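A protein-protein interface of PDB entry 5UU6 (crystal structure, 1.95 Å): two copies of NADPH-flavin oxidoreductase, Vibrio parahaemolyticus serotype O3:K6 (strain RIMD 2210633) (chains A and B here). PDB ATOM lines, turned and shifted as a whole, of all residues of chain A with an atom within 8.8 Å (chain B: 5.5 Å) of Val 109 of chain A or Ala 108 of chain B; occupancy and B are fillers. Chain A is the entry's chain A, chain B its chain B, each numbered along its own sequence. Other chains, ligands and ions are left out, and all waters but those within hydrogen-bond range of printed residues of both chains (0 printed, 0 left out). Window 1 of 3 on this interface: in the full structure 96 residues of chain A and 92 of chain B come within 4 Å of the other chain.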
ATOM      1  N   ALA A  40       9.468  -7.354 -17.474  1.00  0.00           N
ATOM      2  CA  ALA A  40       8.558  -6.545 -16.682  1.00  0.00           C
ATOM      3  C   ALA A  40       8.752  -6.795 -15.185  1.00  0.00           C
ATOM      4  O   ALA A  40       9.119  -7.896 -14.767  1.00  0.00           O
ATOM      5  CB  ALA A  40       7.104  -6.872 -17.069  1.00  0.00           C
ATOM      6  N   SER A  41       8.496  -5.754 -14.373  1.00  0.00           N
ATOM      7  CA  SER A  41       8.388  -5.914 -12.931  1.00  0.00           C
ATOM      8  C   SER A  41       7.390  -7.020 -12.606  1.00  0.00           C
ATOM      9  O   SER A  41       6.456  -7.272 -13.369  1.00  0.00           O
ATOM     10  CB  SER A  41       7.920  -4.610 -12.268  1.00  0.00           C
ATOM     11  OG  SER A  41       8.840  -3.553 -12.500  1.00  0.00           O
ATOM     12  N   SER A  42       7.578  -7.662 -11.447  1.00  0.00           N
ATOM     13  CA  SER A  42       6.735  -8.771 -11.007  1.00  0.00           C
ATOM     14  C   SER A  42       6.508  -8.631  -9.509  1.00  0.00           C
ATOM     15  O   SER A  42       7.477  -8.606  -8.762  1.00  0.00           O
ATOM     16  CB  SER A  42       7.417 -10.121 -11.306  1.00  0.00           C
ATOM     17  OG  SER A  42       6.783 -11.158 -10.578  1.00  0.00           O
ATOM     18  N   SER A  43       5.257  -8.563  -9.057  1.00  0.00           N
ATOM     19  CA  SER A  43       5.028  -8.483  -7.604  1.00  0.00           C
ATOM     20  C   SER A  43       5.697  -9.634  -6.867  1.00  0.00           C
ATOM     21  O   SER A  43       5.416 -10.806  -7.144  1.00  0.00           O
ATOM     22  CB  SER A  43       3.530  -8.504  -7.287  1.00  0.00           C
ATOM     23  OG  SER A  43       2.786  -7.718  -8.191  1.00  0.00           O
ATOM     24  N   VAL A  48       3.766 -14.585 -12.074  1.00  0.00           N
ATOM     25  CA  VAL A  48       2.439 -15.227 -12.050  1.00  0.00           C
ATOM     26  C   VAL A  48       1.781 -15.266 -13.439  1.00  0.00           C
ATOM     27  O   VAL A  48       0.575 -15.517 -13.535  1.00  0.00           O
ATOM     28  CB  VAL A  48       1.506 -14.539 -11.042  1.00  0.00           C
ATOM     29  CG1 VAL A  48       2.052 -14.597  -9.653  1.00  0.00           C
ATOM     30  CG2 VAL A  48       1.345 -13.081 -11.427  1.00  0.00           C
ATOM     31  N   VAL A  49       2.531 -15.018 -14.512  1.00  0.00           N
ATOM     32  CA  VAL A  49       1.939 -14.825 -15.838  1.00  0.00           C
ATOM     33  C   VAL A  49       2.432 -15.921 -16.777  1.00  0.00           C
ATOM     34  O   VAL A  49       3.625 -16.243 -16.811  1.00  0.00           O
ATOM     35  CB  VAL A  49       2.264 -13.434 -16.425  1.00  0.00           C
ATOM     36  CG1 VAL A  49       1.652 -13.259 -17.859  1.00  0.00           C
ATOM     37  CG2 VAL A  49       1.779 -12.319 -15.470  1.00  0.00           C
ATOM     38  N   ILE A  84      -3.244 -15.724 -16.011  1.00  0.00           N
ATOM     39  CA  ILE A  84      -2.760 -15.895 -14.641  1.00  0.00           C
ATOM     40  C   ILE A  84      -2.268 -17.322 -14.439  1.00  0.00           C
ATOM     41  O   ILE A  84      -2.931 -18.293 -14.845  1.00  0.00           O
ATOM     42  CB  ILE A  84      -3.896 -15.583 -13.655  1.00  0.00           C
ATOM     43  CG1 ILE A  84      -4.309 -14.137 -13.795  1.00  0.00           C
ATOM     44  CG2 ILE A  84      -3.454 -15.908 -12.218  1.00  0.00           C
ATOM     45  CD1 ILE A  84      -5.569 -13.821 -12.963  1.00  0.00           C
ATOM     46  N   TYR A  86      -0.825 -19.631 -11.307  1.00  0.00           N
ATOM     47  CA  TYR A  86      -0.344 -20.161 -10.036  1.00  0.00           C
ATOM     48  C   TYR A  86      -0.144 -21.676 -10.095  1.00  0.00           C
ATOM     49  O   TYR A  86       0.069 -22.319  -9.060  1.00  0.00           O
ATOM     50  CB  TYR A  86      -1.293 -19.769  -8.894  1.00  0.00           C
ATOM     51  CG  TYR A  86      -1.222 -18.271  -8.646  1.00  0.00           C
ATOM     52  CD1 TYR A  86      -0.208 -17.737  -7.889  1.00  0.00           C
ATOM     53  CD2 TYR A  86      -2.159 -17.393  -9.216  1.00  0.00           C
ATOM     54  CE1 TYR A  86      -0.119 -16.370  -7.681  1.00  0.00           C
ATOM     55  CE2 TYR A  86      -2.070 -16.013  -9.030  1.00  0.00           C
ATOM     56  CZ  TYR A  86      -1.060 -15.510  -8.258  1.00  0.00           C
ATOM     57  OH  TYR A  86      -0.943 -14.134  -8.054  1.00  0.00           O
ATOM     58  N   THR A 101      -8.341 -13.523  -3.416  1.00  0.00           N
ATOM     59  CA  THR A 101      -8.604 -12.444  -4.394  1.00  0.00           C
ATOM     60  C   THR A 101      -7.370 -11.567  -4.659  1.00  0.00           C
ATOM     61  O   THR A 101      -7.141 -11.119  -5.801  1.00  0.00           O
ATOM     62  CB  THR A 101      -9.762 -11.555  -3.905  1.00  0.00           C
ATOM     63  OG1 THR A 101     -10.976 -12.335  -3.855  1.00  0.00           O
ATOM     64  CG2 THR A 101      -9.980 -10.403  -4.879  1.00  0.00           C
ATOM     65  N   GLU A 102      -6.592 -11.281  -3.610  1.00  0.00           N
ATOM     66  CA  GLU A 102      -5.283 -10.621  -3.681  1.00  0.00           C
ATOM     67  C   GLU A 102      -4.462 -11.165  -4.848  1.00  0.00           C
ATOM     68  O   GLU A 102      -3.801 -10.403  -5.566  1.00  0.00           O
ATOM     69  CB  GLU A 102      -4.549 -10.831  -2.339  1.00  0.00           C
ATOM     70  CG  GLU A 102      -3.033 -10.509  -2.253  1.00  0.00           C
ATOM     71  CD  GLU A 102      -2.663  -9.047  -2.571  1.00  0.00           C
ATOM     72  OE1 GLU A 102      -1.457  -8.722  -2.526  1.00  0.00           O
ATOM     73  OE2 GLU A 102      -3.560  -8.218  -2.822  1.00  0.00           O
ATOM     74  N   LEU A 103      -4.505 -12.480  -5.059  1.00  0.00           N
ATOM     75  CA  LEU A 103      -3.634 -13.072  -6.083  1.00  0.00           C
ATOM     76  C   LEU A 103      -4.194 -12.951  -7.495  1.00  0.00           C
ATOM     77  O   LEU A 103      -3.421 -12.916  -8.460  1.00  0.00           O
ATOM     78  CB  LEU A 103      -3.355 -14.532  -5.756  1.00  0.00           C
ATOM     79  CG  LEU A 103      -2.679 -14.719  -4.371  1.00  0.00           C
ATOM     80  CD1 LEU A 103      -2.843 -16.146  -3.881  1.00  0.00           C
ATOM     81  CD2 LEU A 103      -1.189 -14.297  -4.381  1.00  0.00           C
ATOM     82  N   MET A 104      -5.511 -12.875  -7.649  1.00  0.00           N
ATOM     83  CA  MET A 104      -6.064 -12.596  -8.944  1.00  0.00           C
ATOM     84  C   MET A 104      -5.715 -11.154  -9.284  1.00  0.00           C
ATOM     85  O   MET A 104      -5.373 -10.823 -10.409  1.00  0.00           O
ATOM     86  CB  MET A 104      -7.572 -12.833  -8.965  1.00  0.00           C
ATOM     87  CG  MET A 104      -8.132 -12.712 -10.363  1.00  0.00           C
ATOM     88  SD  MET A 104      -8.744 -10.844 -10.598  1.00  0.00           S
ATOM     89  CE  MET A 104     -10.521 -11.340  -9.902  1.00  0.00           C
ATOM     90  N   LEU A 105      -5.800 -10.292  -8.278  1.00  0.00           N
ATOM     91  CA  LEU A 105      -5.437  -8.897  -8.463  1.00  0.00           C
ATOM     92  C   LEU A 105      -3.984  -8.762  -8.947  1.00  0.00           C
ATOM     93  O   LEU A 105      -3.731  -8.115  -9.955  1.00  0.00           O
ATOM     94  CB  LEU A 105      -5.654  -8.147  -7.156  1.00  0.00           C
ATOM     95  CG  LEU A 105      -5.670  -6.629  -7.175  1.00  0.00           C
ATOM     96  CD1 LEU A 105      -6.389  -6.172  -5.892  1.00  0.00           C
ATOM     97  CD2 LEU A 105      -4.230  -6.035  -7.281  1.00  0.00           C
ATOM     98  N   ILE A 106      -3.035  -9.389  -8.247  1.00  0.00           N
ATOM     99  CA  ILE A 106      -1.625  -9.451  -8.679  1.00  0.00           C
ATOM    100  C   ILE A 106      -1.487 -10.030 -10.080  1.00  0.00           C
ATOM    101  O   ILE A 106      -0.717  -9.517 -10.907  1.00  0.00           O
ATOM    102  CB  ILE A 106      -0.804 -10.280  -7.668  1.00  0.00           C
ATOM    103  CG1 ILE A 106      -0.551  -9.466  -6.410  1.00  0.00           C
ATOM    104  CG2 ILE A 106       0.548 -10.801  -8.262  1.00  0.00           C
ATOM    105  CD1 ILE A 106      -0.160 -10.379  -5.223  1.00  0.00           C
ATOM    106  N   GLY A 107      -2.152 -11.162 -10.336  1.00  0.00           N
ATOM    107  CA  GLY A 107      -2.095 -11.762 -11.673  1.00  0.00           C
ATOM    108  C   GLY A 107      -2.559 -10.802 -12.755  1.00  0.00           C
ATOM    109  O   GLY A 107      -1.938 -10.697 -13.823  1.00  0.00           O
ATOM    110  N   ALA A 108      -3.620 -10.035 -12.472  1.00  0.00           N
ATOM    111  CA  ALA A 108      -4.168  -9.158 -13.499  1.00  0.00           C
ATOM    112  C   ALA A 108      -3.253  -7.972 -13.741  1.00  0.00           C
ATOM    113  O   ALA A 108      -2.968  -7.626 -14.891  1.00  0.00           O
ATOM    114  CB  ALA A 108      -5.570  -8.681 -13.104  1.00  0.00           C
ATOM    115  N   VAL A 109      -2.814  -7.305 -12.666  1.00  0.00           N
ATOM    116  CA  VAL A 109      -1.896  -6.165 -12.824  1.00  0.00           C
ATOM    117  C   VAL A 109      -0.634  -6.606 -13.559  1.00  0.00           C
ATOM    118  O   VAL A 109      -0.204  -5.974 -14.543  1.00  0.00           O
ATOM    119  CB  VAL A 109      -1.555  -5.560 -11.446  1.00  0.00           C
ATOM    120  CG1 VAL A 109      -0.313  -4.695 -11.528  1.00  0.00           C
ATOM    121  CG2 VAL A 109      -2.723  -4.815 -10.881  1.00  0.00           C
ATOM    122  N   ASP A 110      -0.002  -7.687 -13.071  1.00  0.00           N
ATOM    123  CA  ASP A 110       1.261  -8.154 -13.649  1.00  0.00           C
ATOM    124  C   ASP A 110       1.089  -8.569 -15.108  1.00  0.00           C
ATOM    125  O   ASP A 110       1.997  -8.378 -15.920  1.00  0.00           O
ATOM    126  CB  ASP A 110       1.825  -9.326 -12.837  1.00  0.00           C
ATOM    127  CG  ASP A 110       2.414  -8.880 -11.449  1.00  0.00           C
ATOM    128  OD1 ASP A 110       2.006  -7.825 -10.923  1.00  0.00           O
ATOM    129  OD2 ASP A 110       3.308  -9.567 -10.885  1.00  0.00           O
ATOM    130  N   SER A 111      -0.077  -9.106 -15.475  1.00  0.00           N
ATOM    131  CA  SER A 111      -0.336  -9.423 -16.893  1.00  0.00           C
ATOM    132  C   SER A 111      -0.406  -8.162 -17.753  1.00  0.00           C
ATOM    133  O   SER A 111       0.108  -8.133 -18.888  1.00  0.00           O
ATOM    134  CB  SER A 111      -1.659 -10.197 -17.029  1.00  0.00           C
ATOM    135  OG  SER A 111      -1.497 -11.497 -16.483  1.00  0.00           O
ATOM    136  N   GLY A 112      -1.075  -7.124 -17.259  1.00  0.00           N
ATOM    137  CA  GLY A 112      -1.105  -5.875 -18.022  1.00  0.00           C
ATOM    138  C   GLY A 112       0.273  -5.248 -18.180  1.00  0.00           C
ATOM    139  O   GLY A 112       0.596  -4.692 -19.233  1.00  0.00           O
ATOM    140  N   ILE A 113       1.089  -5.286 -17.120  1.00  0.00           N
ATOM    141  CA  ILE A 113       2.465  -4.784 -17.197  1.00  0.00           C
ATOM    142  C   ILE A 113       3.253  -5.544 -18.259  1.00  0.00           C
ATOM    143  O   ILE A 113       3.893  -4.950 -19.140  1.00  0.00           O
ATOM    144  CB  ILE A 113       3.154  -4.897 -15.823  1.00  0.00           C
ATOM    145  CG1 ILE A 113       2.443  -4.069 -14.734  1.00  0.00           C
ATOM    146  CG2 ILE A 113       4.642  -4.483 -15.920  1.00  0.00           C
ATOM    147  CD1 ILE A 113       3.148  -4.263 -13.302  1.00  0.00           C
ATOM    148  N   MET A 114       3.245  -6.868 -18.171  1.00  0.00           N
ATOM    149  CA  MET A 114       3.961  -7.688 -19.173  1.00  0.00           C
ATOM    150  C   MET A 114       3.471  -7.526 -20.638  1.00  0.00           C
ATOM    151  O   MET A 114       4.270  -7.431 -21.596  1.00  0.00           O
ATOM    152  CB  MET A 114       3.861  -9.159 -18.776  1.00  0.00           C
ATOM    153  CG  MET A 114       4.662 -10.031 -19.739  1.00  0.00           C
ATOM    154  SD  MET A 114       4.706 -11.923 -19.261  1.00  0.00           S
ATOM    155  CE  MET A 114       5.835 -11.728 -17.741  1.00  0.00           C
ATOM    156  N   ALA A 115       2.154  -7.568 -20.813  1.00  0.00           N
ATOM    157  CA  ALA A 115       1.557  -7.376 -22.133  1.00  0.00           C
ATOM    158  C   ALA A 115       1.960  -6.041 -22.732  1.00  0.00           C
ATOM    159  O   ALA A 115       2.251  -5.946 -23.938  1.00  0.00           O
ATOM    160  CB  ALA A 115       0.034  -7.436 -22.038  1.00  0.00           C
ATOM    161  N   GLN A 116       1.977  -4.992 -21.907  1.00  0.00           N
ATOM    162  CA  GLN A 116       2.291  -3.674 -22.459  1.00  0.00           C
ATOM    163  C   GLN A 116       3.760  -3.593 -22.855  1.00  0.00           C
ATOM    164  O   GLN A 116       4.096  -2.933 -23.846  1.00  0.00           O
ATOM    165  CB  GLN A 116       1.907  -2.578 -21.449  1.00  0.00           C
ATOM    166  CG  GLN A 116       2.107  -1.129 -21.977  1.00  0.00           C
ATOM    167  CD  GLN A 116       1.312  -0.780 -23.235  1.00  0.00           C
ATOM    168  OE1 GLN A 116       0.329  -1.468 -23.610  1.00  0.00           O
ATOM    169  NE2 GLN A 116       1.736   0.298 -23.911  1.00  0.00           N
ATOM    170  N   LEU A 155      -6.977 -14.159 -19.293  1.00  0.00           N
ATOM    171  CA  LEU A 155      -7.362 -12.774 -19.044  1.00  0.00           C
ATOM    172  C   LEU A 155      -7.635 -12.026 -20.334  1.00  0.00           C
ATOM    173  O   LEU A 155      -8.684 -11.389 -20.452  1.00  0.00           O
ATOM    174  CB  LEU A 155      -6.252 -12.044 -18.281  1.00  0.00           C
ATOM    175  CG  LEU A 155      -6.088 -12.463 -16.842  1.00  0.00           C
ATOM    176  CD1 LEU A 155      -5.060 -11.515 -16.217  1.00  0.00           C
ATOM    177  CD2 LEU A 155      -7.452 -12.425 -16.104  1.00  0.00           C
ATOM    178  N   PHE A 156      -6.710 -12.063 -21.307  1.00  0.00           N
ATOM    179  CA  PHE A 156      -6.958 -11.391 -22.586  1.00  0.00           C
ATOM    180  C   PHE A 156      -5.957 -11.910 -23.605  1.00  0.00           C
ATOM    181  O   PHE A 156      -4.920 -12.501 -23.268  1.00  0.00           O
ATOM    182  CB  PHE A 156      -6.829  -9.858 -22.467  1.00  0.00           C
ATOM    183  CG  PHE A 156      -5.504  -9.433 -21.903  1.00  0.00           C
ATOM    184  CD1 PHE A 156      -4.402  -9.267 -22.740  1.00  0.00           C
ATOM    185  CD2 PHE A 156      -5.329  -9.293 -20.524  1.00  0.00           C
ATOM    186  CE1 PHE A 156      -3.135  -8.928 -22.209  1.00  0.00           C
ATOM    187  CE2 PHE A 156      -4.057  -8.949 -19.983  1.00  0.00           C
ATOM    188  CZ  PHE A 156      -2.966  -8.770 -20.839  1.00  0.00           C
ATOM    189  N   ILE B  84      -8.453   1.865  -9.233  1.00  0.00           N
ATOM    190  CA  ILE B  84      -9.607   1.544 -10.072  1.00  0.00           C
ATOM    191  C   ILE B  84     -10.654   2.622  -9.865  1.00  0.00           C
ATOM    192  O   ILE B  84     -10.959   2.987  -8.727  1.00  0.00           O
ATOM    193  CB  ILE B  84     -10.221   0.175  -9.721  1.00  0.00           C
ATOM    194  CG1 ILE B  84      -9.221  -0.958  -9.837  1.00  0.00           C
ATOM    195  CG2 ILE B  84     -11.431  -0.119 -10.631  1.00  0.00           C
ATOM    196  CD1 ILE B  84      -9.784  -2.313  -9.277  1.00  0.00           C
ATOM    197  N   LEU B 103     -15.291  -6.249 -13.757  1.00  0.00           N
ATOM    198  CA  LEU B 103     -14.856  -4.856 -13.794  1.00  0.00           C
ATOM    199  C   LEU B 103     -13.630  -4.611 -12.926  1.00  0.00           C
ATOM    200  O   LEU B 103     -12.859  -3.679 -13.190  1.00  0.00           O
ATOM    201  CB  LEU B 103     -16.004  -3.932 -13.391  1.00  0.00           C
ATOM    202  CG  LEU B 103     -17.182  -4.096 -14.376  1.00  0.00           C
ATOM    203  CD1 LEU B 103     -18.348  -3.264 -13.901  1.00  0.00           C
ATOM    204  CD2 LEU B 103     -16.788  -3.718 -15.786  1.00  0.00           C
ATOM    205  N   MET B 104     -13.423  -5.411 -11.901  1.00  0.00           N
ATOM    206  CA  MET B 104     -12.183  -5.305 -11.153  1.00  0.00           C
ATOM    207  C   MET B 104     -10.990  -5.871 -11.981  1.00  0.00           C
ATOM    208  O   MET B 104      -9.892  -5.318 -11.921  1.00  0.00           O
ATOM    209  CB  MET B 104     -12.363  -5.998  -9.796  1.00  0.00           C
ATOM    210  CG  MET B 104     -11.300  -5.622  -8.734  1.00  0.00           C
ATOM    211  SD  MET B 104      -9.683  -6.750  -9.038  1.00  0.00           S
ATOM    212  CE  MET B 104     -10.659  -8.222  -9.670  1.00  0.00           C
ATOM    213  N   LEU B 105     -11.205  -6.984 -12.711  1.00  0.00           N
ATOM    214  CA  LEU B 105     -10.197  -7.506 -13.637  1.00  0.00           C
ATOM    215  C   LEU B 105      -9.751  -6.427 -14.617  1.00  0.00           C
ATOM    216  O   LEU B 105      -8.554  -6.197 -14.820  1.00  0.00           O
ATOM    217  CB  LEU B 105     -10.790  -8.655 -14.428  1.00  0.00           C
ATOM    218  CG  LEU B 105     -10.805 -10.119 -14.103  1.00  0.00           C
ATOM    219  CD1 LEU B 105     -11.105 -10.878 -15.407  1.00  0.00           C
ATOM    220  CD2 LEU B 105      -9.433 -10.442 -13.637  1.00  0.00           C
ATOM    221  N   ILE B 106     -10.732  -5.775 -15.244  1.00  0.00           N
ATOM    222  CA  ILE B 106     -10.481  -4.707 -16.202  1.00  0.00           C
ATOM    223  C   ILE B 106      -9.697  -3.582 -15.538  1.00  0.00           C
ATOM    224  O   ILE B 106      -8.695  -3.094 -16.076  1.00  0.00           O
ATOM    225  CB  ILE B 106     -11.834  -4.227 -16.784  1.00  0.00           C
ATOM    226  CG1 ILE B 106     -12.347  -5.195 -17.849  1.00  0.00           C
ATOM    227  CG2 ILE B 106     -11.793  -2.778 -17.323  1.00  0.00           C
ATOM    228  CD1 ILE B 106     -13.784  -4.836 -18.320  1.00  0.00           C
ATOM    229  N   GLY B 107     -10.136  -3.150 -14.350  1.00  0.00           N
ATOM    230  CA  GLY B 107      -9.425  -2.068 -13.676  1.00  0.00           C
ATOM    231  C   GLY B 107      -8.001  -2.462 -13.324  1.00  0.00           C
ATOM    232  O   GLY B 107      -7.065  -1.664 -13.489  1.00  0.00           O
ATOM    233  N   ALA B 108      -7.804  -3.724 -12.911  1.00  0.00           N
ATOM    234  CA  ALA B 108      -6.470  -4.202 -12.567  1.00  0.00           C
ATOM    235  C   ALA B 108      -5.578  -4.279 -13.798  1.00  0.00           C
ATOM    236  O   ALA B 108      -4.442  -3.771 -13.779  1.00  0.00           O
ATOM    237  CB  ALA B 108      -6.555  -5.565 -11.889  1.00  0.00           C
ATOM    238  N   VAL B 109      -6.081  -4.870 -14.895  1.00  0.00           N
ATOM    239  CA  VAL B 109      -5.251  -5.001 -16.101  1.00  0.00           C
ATOM    240  C   VAL B 109      -4.907  -3.630 -16.654  1.00  0.00           C
ATOM    241  O   VAL B 109      -3.731  -3.326 -16.955  1.00  0.00           O
ATOM    242  CB  VAL B 109      -5.941  -5.875 -17.170  1.00  0.00           C
ATOM    243  CG1 VAL B 109      -5.252  -5.692 -18.553  1.00  0.00           C
ATOM    244  CG2 VAL B 109      -5.912  -7.314 -16.805  1.00  0.00           C
ATOM    245  N   ASP B 110      -5.922  -2.767 -16.782  1.00  0.00           N
ATOM    246  CA  ASP B 110      -5.698  -1.454 -17.376  1.00  0.00           C
ATOM    247  C   ASP B 110      -4.763  -0.608 -16.525  1.00  0.00           C
ATOM    248  O   ASP B 110      -3.949   0.153 -17.070  1.00  0.00           O
ATOM    249  CB  ASP B 110      -7.032  -0.738 -17.612  1.00  0.00           C
ATOM    250  CG  ASP B 110      -7.867  -1.390 -18.786  1.00  0.00           C
ATOM    251  OD1 ASP B 110      -7.588  -2.570 -19.153  1.00  0.00           O
ATOM    252  OD2 ASP B 110      -8.789  -0.716 -19.341  1.00  0.00           O
ATOM    253  N   SER B 111      -4.823  -0.764 -15.191  1.00  0.00           N
ATOM    254  CA  SER B 111      -3.889  -0.054 -14.330  1.00  0.00           C
ATOM    255  C   SER B 111      -2.463  -0.511 -14.598  1.00  0.00           C
ATOM    256  O   SER B 111      -1.548   0.311 -14.642  1.00  0.00           O
ATOM    257  CB  SER B 111      -4.234  -0.292 -12.859  1.00  0.00           C
ATOM    258  OG  SER B 111      -5.428   0.436 -12.515  1.00  0.00           O
ATOM    259  N   GLY B 112      -2.248  -1.822 -14.774  1.00  0.00           N
ATOM    260  CA  GLY B 112      -0.898  -2.288 -15.048  1.00  0.00           C
ATOM    261  C   GLY B 112      -0.375  -1.775 -16.378  1.00  0.00           C
ATOM    262  O   GLY B 112       0.799  -1.406 -16.497  1.00  0.00           O
ATOM    263  N   ILE B 113      -1.254  -1.684 -17.377  1.00  0.00           N
ATOM    264  CA  ILE B 113      -0.873  -1.178 -18.690  1.00  0.00           C
ATOM    265  C   ILE B 113      -0.470   0.285 -18.601  1.00  0.00           C
ATOM    266  O   ILE B 113       0.548   0.691 -19.150  1.00  0.00           O
ATOM    267  CB  ILE B 113      -2.028  -1.370 -19.685  1.00  0.00           C
ATOM    268  CG1 ILE B 113      -2.283  -2.865 -19.927  1.00  0.00           C
ATOM    269  CG2 ILE B 113      -1.754  -0.628 -21.035  1.00  0.00           C
ATOM    270  CD1 ILE B 113      -3.499  -3.088 -20.818  1.00  0.00           C
ATOM    271  N   LEU B 155      -4.862   0.211  -5.939  1.00  0.00           N
ATOM    272  CA  LEU B 155      -4.209  -1.012  -6.405  1.00  0.00           C
ATOM    273  C   LEU B 155      -2.734  -1.040  -6.062  1.00  0.00           C
ATOM    274  O   LEU B 155      -2.244  -2.051  -5.519  1.00  0.00           O
ATOM    275  CB  LEU B 155      -4.366  -1.187  -7.924  1.00  0.00           C
ATOM    276  CG  LEU B 155      -5.791  -1.460  -8.422  1.00  0.00           C
ATOM    277  CD1 LEU B 155      -5.787  -1.675  -9.915  1.00  0.00           C
ATOM    278  CD2 LEU B 155      -6.403  -2.655  -7.711  1.00  0.00           C
ATOM    279  N   PHE B 156      -2.001   0.034  -6.368  1.00  0.00           N
ATOM    280  CA  PHE B 156      -0.580   0.059  -6.053  1.00  0.00           C
ATOM    281  C   PHE B 156      -0.091   1.478  -6.259  1.00  0.00           C
ATOM    282  O   PHE B 156      -0.751   2.291  -6.919  1.00  0.00           O
ATOM    283  CB  PHE B 156       0.231  -0.909  -6.920  1.00  0.00           C
ATOM    284  CG  PHE B 156       0.047  -0.693  -8.405  1.00  0.00           C
ATOM    285  CD1 PHE B 156       0.850   0.227  -9.104  1.00  0.00           C
ATOM    286  CD2 PHE B 156      -0.919  -1.399  -9.097  1.00  0.00           C
ATOM    287  CE1 PHE B 156       0.685   0.447 -10.481  1.00  0.00           C
ATOM    288  CE2 PHE B 156      -1.134  -1.155 -10.500  1.00  0.00           C
ATOM    289  CZ  PHE B 156      -0.312  -0.245 -11.179  1.00  0.00           C
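Met 104 of chain A touches Met 104 of chain B.
Ala 108 of chain B touches Ala 108 of chain A.
O of Ala 108 of chain A touches CG2 of Val 109 of chain B (3.5 Å).
Val 109 of chain A touches Ala 108 of chain B.
O of Val 109 of chain A touches CA of Gly 112 of chain B, 3.8 Å away.
CA of Gly 112 of chain A touches O of Val 109 of chain B, 3.8 Å away.
O of Gly 112 of chain A touches CG1 of Ile 113 of chain B (3.5 Å).
Gln 116 of chain A touches Ile 113 of chain B.
Leu 155 of chain A touches Leu 105 of chain B (CD2 to CD2, 3.7 Å).
CE2 of Phe 156 of chain A touches CG1 of Val 109 of chain B (3.8 Å).
Ile 84 of chain A touches none of the printed residues of chain B.
Thr 101 of chain A touches none of the printed residues of chain B.
Of the printed residues of chain B, Leu 105 of chain A touches Leu 155.
Val 109 of chain A touches just these residues of chain B: Ala 108, Gly 112 and Phe 156.
Of the printed residues of chain B, Gly 112 of chain A touches Val 109 (3.8 Å), Gly 112 (3.97 Å) and Ile 113 (3.5 Å).
No residue of chain A comes within 4 Å of Gly 107 of chain B.
Of the printed residues of chain A, Gly 112 of chain B touches Val 109 (3.8 Å), Gly 112 (3.97 Å) and Ile 113 (3.6 Å).
Printed residues of chain A within 4 Å of Leu 155 of chain B: Leu 105 (3.96 Å).
Of the printed residues of chain A, Phe 156 of chain B touches Val 109.
The nearest printed residue of chain A that does not touch Leu 155 of chain B is Val 109 of chain A (4.5 Å).
Of the 14 printed residues of chain B, 8 touch a printed residue of chain A.
Printed residues of chain B that touch a printed residue of chain A: Met 104, Leu 105, Ala 108, Val 109, Gly 112, Ile 113, Leu 155 and Phe 156.
Hydrophobic or aromatic side chains of chain B that line the printed part of chain A: Met 104, Leu 105, Ala 108, Val 109, Ile 113, Leu 155 and Phe 156.
Among the printed residues, no Asp or Glu carboxylate lies within 4 Å of a Lys or Arg side-chain nitrogen of the other chain.
Met 104 of chain A touches Leu 105 of chain B, but with the chains exchanged Leu 105 of chain A does not touch Met 104 of chain B (4.4 Å).
Leu 105 of chain A touches Leu 155 of chain B, and with the chains exchanged Leu 155 of chain A touches Leu 105 of chain B.
Ala 108 of chain A touches Val 109 of chain B, and with the chains exchanged Val 109 of chain A touches Ala 108 of chain B.
Val 109 of chain A touches Phe 156 of chain B, and with the chains exchanged Phe 156 of chain A touches Val 109 of chain B.
Positions printed for both chains: 84, 103, 104, 105, 106, 107, 108, 109, 110, 111, 112, 113, 155 and 156.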
